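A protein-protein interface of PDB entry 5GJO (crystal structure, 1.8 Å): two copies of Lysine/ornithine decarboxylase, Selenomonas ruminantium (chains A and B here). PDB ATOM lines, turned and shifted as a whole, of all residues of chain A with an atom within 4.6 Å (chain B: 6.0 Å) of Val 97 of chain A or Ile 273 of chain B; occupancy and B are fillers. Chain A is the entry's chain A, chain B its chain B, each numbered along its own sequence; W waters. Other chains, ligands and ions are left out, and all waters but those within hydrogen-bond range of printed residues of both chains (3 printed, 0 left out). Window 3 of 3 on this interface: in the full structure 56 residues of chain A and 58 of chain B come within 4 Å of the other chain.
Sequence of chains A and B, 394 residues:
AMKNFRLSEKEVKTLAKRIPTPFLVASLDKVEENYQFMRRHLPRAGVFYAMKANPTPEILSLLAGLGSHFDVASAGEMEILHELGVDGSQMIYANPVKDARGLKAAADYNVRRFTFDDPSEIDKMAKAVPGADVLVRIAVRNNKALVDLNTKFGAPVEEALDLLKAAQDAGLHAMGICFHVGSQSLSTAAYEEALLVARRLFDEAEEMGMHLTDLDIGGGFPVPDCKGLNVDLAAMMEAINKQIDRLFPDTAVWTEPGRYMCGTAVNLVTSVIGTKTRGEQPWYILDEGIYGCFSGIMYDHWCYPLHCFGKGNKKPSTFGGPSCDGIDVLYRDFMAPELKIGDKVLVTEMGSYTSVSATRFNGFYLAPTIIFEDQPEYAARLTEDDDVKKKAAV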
ATOM      1  N   ASN A  95       5.957 -29.635   4.902  1.00  0.00           N
ATOM      2  CA  ASN A  95       5.380 -30.389   3.789  1.00  0.00           C
ATOM      3  C   ASN A  95       5.905 -29.723   2.525  1.00  0.00           C
ATOM      4  O   ASN A  95       5.595 -28.523   2.290  1.00  0.00           O
ATOM      5  CB  ASN A  95       3.931 -30.335   3.863  1.00  0.00           C
ATOM      6  CG  ASN A  95       3.248 -31.333   2.944  1.00  0.00           C
ATOM      7  OD1 ASN A  95       3.742 -31.634   1.844  1.00  0.00           O
ATOM      8  ND2 ASN A  95       2.130 -31.923   3.440  1.00  0.00           N
ATOM      9  N   PRO A  96       6.699 -30.464   1.744  1.00  0.00           N
ATOM     10  CA  PRO A  96       7.261 -29.816   0.559  1.00  0.00           C
ATOM     11  C   PRO A  96       6.209 -29.378  -0.448  1.00  0.00           C
ATOM     12  O   PRO A  96       6.581 -28.541  -1.276  1.00  0.00           O
ATOM     13  CB  PRO A  96       8.177 -30.910  -0.058  1.00  0.00           C
ATOM     14  CG  PRO A  96       8.422 -31.851   1.046  1.00  0.00           C
ATOM     15  CD  PRO A  96       7.160 -31.843   1.858  1.00  0.00           C
ATOM     16  N   VAL A  97       5.016 -29.961  -0.474  1.00  0.00           N
ATOM     17  CA  VAL A  97       4.004 -29.615  -1.425  1.00  0.00           C
ATOM     18  C   VAL A  97       2.816 -29.137  -0.696  1.00  0.00           C
ATOM     19  O   VAL A  97       1.987 -29.909  -0.273  1.00  0.00           O
ATOM     20  CB  VAL A  97       3.675 -30.735  -2.413  1.00  0.00           C
ATOM     21  CG1 VAL A  97       2.641 -30.229  -3.456  1.00  0.00           C
ATOM     22  CG2 VAL A  97       4.953 -31.223  -3.078  1.00  0.00           C
ATOM     23  N   LYS A  98       2.654 -27.826  -0.640  1.00  0.00           N
ATOM     24  CA  LYS A  98       1.604 -27.235   0.204  1.00  0.00           C
ATOM     25  C   LYS A  98       0.282 -27.027  -0.495  1.00  0.00           C
ATOM     26  O   LYS A  98       0.285 -26.829  -1.698  1.00  0.00           O
ATOM     27  CB  LYS A  98       2.143 -25.946   0.752  1.00  0.00           C
ATOM     28  CG  LYS A  98       3.388 -26.161   1.595  1.00  0.00           C
ATOM     29  CD  LYS A  98       4.259 -24.904   1.644  1.00  0.00           C
ATOM     30  CE  LYS A  98       5.710 -25.211   1.932  1.00  0.00           C
ATOM     31  NZ  LYS A  98       6.258 -26.186   0.925  1.00  0.00           N
ATOM     32  N   ASP A  99      -0.829 -27.068   0.220  1.00  0.00           N
ATOM     33  CA  ASP A  99      -2.118 -26.779  -0.389  1.00  0.00           C
ATOM     34  C   ASP A  99      -2.592 -25.382  -0.014  1.00  0.00           C
ATOM     35  O   ASP A  99      -1.950 -24.690   0.736  1.00  0.00           O
ATOM     36  CB  ASP A  99      -3.165 -27.861  -0.110  1.00  0.00           C
ATOM     37  CG  ASP A  99      -3.616 -27.880   1.327  1.00  0.00           C
ATOM     38  OD1 ASP A  99      -3.161 -27.038   2.089  1.00  0.00           O
ATOM     39  OD2 ASP A  99      -4.429 -28.731   1.687  1.00  0.00           O
ATOM     40  N   GLU A 121       6.874 -25.271  -6.551  1.00  0.00           N
ATOM     41  CA  GLU A 121       6.521 -24.811  -5.204  1.00  0.00           C
ATOM     42  C   GLU A 121       6.849 -23.341  -4.927  1.00  0.00           C
ATOM     43  O   GLU A 121       6.316 -22.731  -4.031  1.00  0.00           O
ATOM     44  CB  GLU A 121       7.226 -25.671  -4.166  1.00  0.00           C
ATOM     45  CG  GLU A 121       6.651 -25.564  -2.753  1.00  0.00           C
ATOM     46  CD  GLU A 121       5.279 -26.191  -2.590  1.00  0.00           C
ATOM     47  OE1 GLU A 121       4.778 -26.770  -3.559  1.00  0.00           O
ATOM     48  OE2 GLU A 121       4.714 -26.095  -1.495  1.00  0.00           O
ATOM     49  N   LYS A 124       3.997 -20.437  -5.403  1.00  0.00           N
ATOM     50  CA  LYS A 124       2.989 -20.625  -4.351  1.00  0.00           C
ATOM     51  C   LYS A 124       3.512 -20.025  -3.036  1.00  0.00           C
ATOM     52  O   LYS A 124       2.757 -19.300  -2.367  1.00  0.00           O
ATOM     53  CB  LYS A 124       2.682 -22.151  -4.096  1.00  0.00           C
ATOM     54  CG  LYS A 124       1.954 -22.883  -5.181  1.00  0.00           C
ATOM     55  CD  LYS A 124       2.114 -24.452  -5.117  1.00  0.00           C
ATOM     56  CE  LYS A 124       1.673 -25.029  -3.827  1.00  0.00           C
ATOM     57  NZ  LYS A 124       1.827 -26.540  -3.772  1.00  0.00           N
ATOM     58  N   SER B 271      -7.829 -31.558  -6.569  1.00  0.00           N
ATOM     59  CA  SER B 271      -6.944 -30.617  -7.344  1.00  0.00           C
ATOM     60  C   SER B 271      -5.530 -31.069  -7.360  1.00  0.00           C
ATOM     61  O   SER B 271      -5.020 -31.567  -6.316  1.00  0.00           O
ATOM     62  CB  SER B 271      -6.962 -29.178  -6.804  1.00  0.00           C
ATOM     63  OG  SER B 271      -8.257 -28.648  -6.850  1.00  0.00           O
ATOM     64  N   VAL B 272      -4.859 -30.816  -8.495  1.00  0.00           N
ATOM     65  CA  VAL B 272      -3.438 -30.925  -8.552  1.00  0.00           C
ATOM     66  C   VAL B 272      -2.871 -29.747  -7.731  1.00  0.00           C
ATOM     67  O   VAL B 272      -3.197 -28.577  -8.032  1.00  0.00           O
ATOM     68  CB  VAL B 272      -2.943 -30.819 -10.031  1.00  0.00           C
ATOM     69  CG1 VAL B 272      -1.440 -30.776 -10.056  1.00  0.00           C
ATOM     70  CG2 VAL B 272      -3.481 -32.015 -10.793  1.00  0.00           C
ATOM     71  N   ILE B 273      -2.092 -30.025  -6.663  1.00  0.00           N
ATOM     72  CA  ILE B 273      -1.424 -29.002  -5.900  1.00  0.00           C
ATOM     73  C   ILE B 273       0.052 -28.887  -6.158  1.00  0.00           C
ATOM     74  O   ILE B 273       0.736 -27.944  -5.710  1.00  0.00           O
ATOM     75  CB  ILE B 273      -1.697 -29.114  -4.342  1.00  0.00           C
ATOM     76  CG1 ILE B 273      -1.177 -30.452  -3.792  1.00  0.00           C
ATOM     77  CG2 ILE B 273      -3.163 -28.998  -4.035  1.00  0.00           C
ATOM     78  CD1 ILE B 273      -1.295 -30.558  -2.262  1.00  0.00           C
ATOM     79  N   GLY B 274       0.645 -29.826  -6.891  1.00  0.00           N
ATOM     80  CA  GLY B 274       2.038 -29.705  -7.160  1.00  0.00           C
ATOM     81  C   GLY B 274       2.385 -30.607  -8.345  1.00  0.00           C
ATOM     82  O   GLY B 274       1.642 -31.589  -8.652  1.00  0.00           O
ATOM     83  N   THR B 275       3.417 -30.217  -9.089  1.00  0.00           N
ATOM     84  CA  THR B 275       3.943 -31.042 -10.150  1.00  0.00           C
ATOM     85  C   THR B 275       5.400 -31.338  -9.870  1.00  0.00           C
ATOM     86  O   THR B 275       6.092 -30.621  -9.118  1.00  0.00           O
ATOM     87  CB  THR B 275       3.838 -30.385 -11.563  1.00  0.00           C
ATOM     88  OG1 THR B 275       4.701 -29.263 -11.554  1.00  0.00           O
ATOM     89  CG2 THR B 275       2.486 -30.004 -11.881  1.00  0.00           C
ATOM     90  N   LYS B 276       5.879 -32.406 -10.483  1.00  0.00           N
ATOM     91  CA  LYS B 276       7.307 -32.708 -10.559  1.00  0.00           C
ATOM     92  C   LYS B 276       7.614 -33.161 -12.013  1.00  0.00           C
ATOM     93  O   LYS B 276       7.186 -34.268 -12.428  1.00  0.00           O
ATOM     94  CB  LYS B 276       7.780 -33.756  -9.576  1.00  0.00           C
ATOM     95  CG  LYS B 276       7.335 -33.500  -8.190  1.00  0.00           C
ATOM     96  CD  LYS B 276       7.554 -34.679  -7.266  1.00  0.00           C
ATOM     97  CE  LYS B 276       7.029 -34.249  -5.886  1.00  0.00           C
ATOM     98  NZ  LYS B 276       7.520 -32.958  -5.257  1.00  0.00           N
ATOM     99  N   ILE B 285       0.887 -34.193  -7.595  1.00  0.00           N
ATOM    100  CA  ILE B 285       0.431 -34.329  -6.216  1.00  0.00           C
ATOM    101  C   ILE B 285      -0.971 -33.747  -6.086  1.00  0.00           C
ATOM    102  O   ILE B 285      -1.272 -32.635  -6.540  1.00  0.00           O
ATOM    103  CB  ILE B 285       1.419 -33.644  -5.257  1.00  0.00           C
ATOM    104  CG1 ILE B 285       2.831 -34.103  -5.484  1.00  0.00           C
ATOM    105  CG2 ILE B 285       0.954 -33.816  -3.815  1.00  0.00           C
ATOM    106  CD1 ILE B 285       3.061 -35.609  -5.266  1.00  0.00           C
ATOM    107  N   LEU B 286      -1.846 -34.560  -5.511  1.00  0.00           N
ATOM    108  CA  LEU B 286      -3.262 -34.285  -5.368  1.00  0.00           C
ATOM    109  C   LEU B 286      -3.561 -33.907  -3.928  1.00  0.00           C
ATOM    110  O   LEU B 286      -2.807 -34.256  -3.050  1.00  0.00           O
ATOM    111  CB  LEU B 286      -4.085 -35.510  -5.732  1.00  0.00           C
ATOM    112  CG  LEU B 286      -3.981 -36.049  -7.166  1.00  0.00           C
ATOM    113  CD1 LEU B 286      -5.026 -37.120  -7.401  1.00  0.00           C
ATOM    114  CD2 LEU B 286      -4.160 -34.903  -8.141  1.00  0.00           C
ATOM    115  N   ASP B 287      -4.669 -33.211  -3.713  1.00  0.00           N
ATOM    116  CA  ASP B 287      -5.022 -32.787  -2.366  1.00  0.00           C
ATOM    117  C   ASP B 287      -5.852 -33.800  -1.582  1.00  0.00           C
ATOM    118  O   ASP B 287      -6.336 -33.492  -0.514  1.00  0.00           O
ATOM    119  CB  ASP B 287      -5.585 -31.357  -2.257  1.00  0.00           C
ATOM    120  CG  ASP B 287      -6.843 -31.110  -3.087  1.00  0.00           C
ATOM    121  OD1 ASP B 287      -7.440 -32.020  -3.640  1.00  0.00           O
ATOM    122  OD2 ASP B 287      -7.244 -29.947  -3.159  1.00  0.00           O
ATOM    123  N   PRO B 322      -1.237 -35.833  -0.701  1.00  0.00           N
ATOM    124  CA  PRO B 322      -0.708 -34.637  -0.103  1.00  0.00           C
ATOM    125  C   PRO B 322       0.086 -34.874   1.197  1.00  0.00           C
ATOM    126  O   PRO B 322       0.706 -33.966   1.718  1.00  0.00           O
ATOM    127  CB  PRO B 322      -1.974 -33.838   0.186  1.00  0.00           C
ATOM    128  CG  PRO B 322      -2.925 -34.906   0.615  1.00  0.00           C
ATOM    129  CD  PRO B 322      -2.653 -36.011  -0.415  1.00  0.00           C
ATOM    130  N   ILE B 341      -0.765 -27.188 -11.836  1.00  0.00           N
ATOM    131  CA  ILE B 341      -1.304 -26.815 -10.532  1.00  0.00           C
ATOM    132  C   ILE B 341      -2.623 -26.060 -10.703  1.00  0.00           C
ATOM    133  O   ILE B 341      -2.760 -25.132 -11.553  1.00  0.00           O
ATOM    134  CB  ILE B 341      -0.300 -26.005  -9.717  1.00  0.00           C
ATOM    135  CG1 ILE B 341       0.897 -26.903  -9.341  1.00  0.00           C
ATOM    136  CG2 ILE B 341      -0.992 -25.415  -8.481  1.00  0.00           C
ATOM    137  CD1 ILE B 341       2.117 -26.175  -8.836  1.00  0.00           C
ATOM    138  N   GLY B 342      -3.642 -26.529  -9.971  1.00  0.00           N
ATOM    139  CA  GLY B 342      -4.994 -26.016 -10.055  1.00  0.00           C
ATOM    140  C   GLY B 342      -5.994 -26.771 -10.890  1.00  0.00           C
ATOM    141  O   GLY B 342      -7.172 -26.580 -10.684  1.00  0.00           O
ATOM    142  N   ASP B 343      -5.520 -27.644 -11.790  1.00  0.00           N
ATOM    143  CA  ASP B 343      -6.335 -28.504 -12.571  1.00  0.00           C
ATOM    144  C   ASP B 343      -7.067 -29.476 -11.629  1.00  0.00           C
ATOM    145  O   ASP B 343      -6.525 -29.860 -10.585  1.00  0.00           O
ATOM    146  CB  ASP B 343      -5.506 -29.319 -13.589  1.00  0.00           C
ATOM    147  CG  ASP B 343      -4.955 -28.519 -14.752  1.00  0.00           C
ATOM    148  OD1 ASP B 343      -5.287 -27.354 -14.837  1.00  0.00           O
ATOM    149  OD2 ASP B 343      -4.202 -29.107 -15.588  1.00  0.00           O
HETATM  150  O   HOH W   1      -5.810 -31.608   1.382  1.00  0.00           O
HETATM  151  O   HOH W   2      -0.203 -30.819   1.240  1.00  0.00           O
HETATM  152  O   HOH W   3       3.485 -33.760   0.167  1.00  0.00           O
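Water W3 lies within hydrogen-bond range of the side-chain amide oxygen (OD1) of Asn 95 of chain A (2.7 Å) and the backbone carbonyl oxygen (O) of Pro 322 of chain B (3.2 Å).
Water W1 lies within hydrogen-bond range of O of Asp 287 of chain B and OD2 of Asp 99 of chain A.
Water W2 lies within hydrogen-bond range of the backbone carbonyl oxygen (O) of Val 97 of chain A (2.8 Å), the backbone carbonyl oxygen (O) of Pro 322 of chain B (3.3 Å) and the side-chain amide nitrogen (ND2) of Asn 95 of chain A (3.4 Å).
ND2 of Asn 95 of chain A lies within hydrogen-bond range of O of Pro 322 of chain B, at 3.0 Å.
NZ of Lys 124 of chain A lies within hydrogen-bond range of O of Ile 273 of chain B (2.6 Å).
Of the 13 printed residues of chain B, 5 touch a printed residue of chain A.
Hydrophobic or aromatic side chains of chain B within 4 Å of the printed part of chain A: Ile 273 and Ile 285.
Hydrophobic or aromatic side chains of chain A that line the printed part of chain B: Val 97.
Among the printed residues, 7 pairs touch across the chains.
Among the printed residues, no Asp or Glu carboxylate lies within 4 Å of a Lys or Arg side-chain nitrogen of the other chain.
No position is printed for both chains.
Of the 7 pairs that touch across the chains among the printed residues, none has its exchanged pair printed and touching as well.
Printed residues of chain B within 4 Å of Asn 95 of chain A: Pro 322.
Of the printed residues of chain B, Val 97 of chain A touches Ile 273, Gly 274, Lys 276 and Ile 285.
Glu 121 of chain A touches none of the printed residues of chain B.
Of the printed residues of chain B, Lys 124 of chain A touches Ile 273.
Printed residues of chain A within 4 Å of Ile 273 of chain B: Val 97, Asp 99 and Lys 124.
Of the printed residues of chain A, Lys 276 of chain B touches Val 97.
Of the printed residues of chain A, Ile 285 of chain B touches Val 97 (3.98 Å).
Of the printed residues of chain A, Pro 322 of chain B touches Asn 95.
The nearest printed residue of chain A that does not touch Ile 273 of chain B is Lys 98 of chain A (4.02 Å).
The nearest printed residue of chain B that does not touch Asn 95 of chain A is Ile 273 of chain B (6.6 Å).
Among the printed residues, pairs that only touch across the chains: Val 97 of chain A with Ile 273 of chain B (3.7 Å), Val 97 of chain A with Lys 276 of chain B (3.8 Å), Val 97 of chain A with Gly 274 of chain B (3.8 Å), Asp 99 of chain A with Ile 273 of chain B (3.9 Å) and Val 97 of chain A with Ile 285 of chain B (3.98 Å).
OD1 of Asn 95 of chain A sits at hydrogen-bond distance from N of Val 97 of chain A (3.1 Å).
The side-chain amino group (NZ) of Lys 124 of chain A lies within hydrogen-bond range of the backbone carbonyl oxygen (O) of Lys 98 of chain A, 2.6 Å away.
The backbone carbonyl oxygen (O) of Gly 274 of chain B is in hydrogen-bond range of the backbone NH (N) of Ile 285 of chain B (2.9 Å).
The backbone carbonyl oxygen (O) of Asn 95 of chain A sits at hydrogen-bond distance from the side-chain amino group (NZ) of Lys 98 of chain A (2.8 Å).
The side-chain carboxylate of Glu 121 of chain A lies within salt-bridge range of the side-chain amino group of Lys 124 of chain A (3.0 Å).
The backbone NH (N) of Ile 273 of chain B lies within hydrogen-bond range of the backbone carbonyl oxygen (O) of Ile 285 of chain B (2.7 Å).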
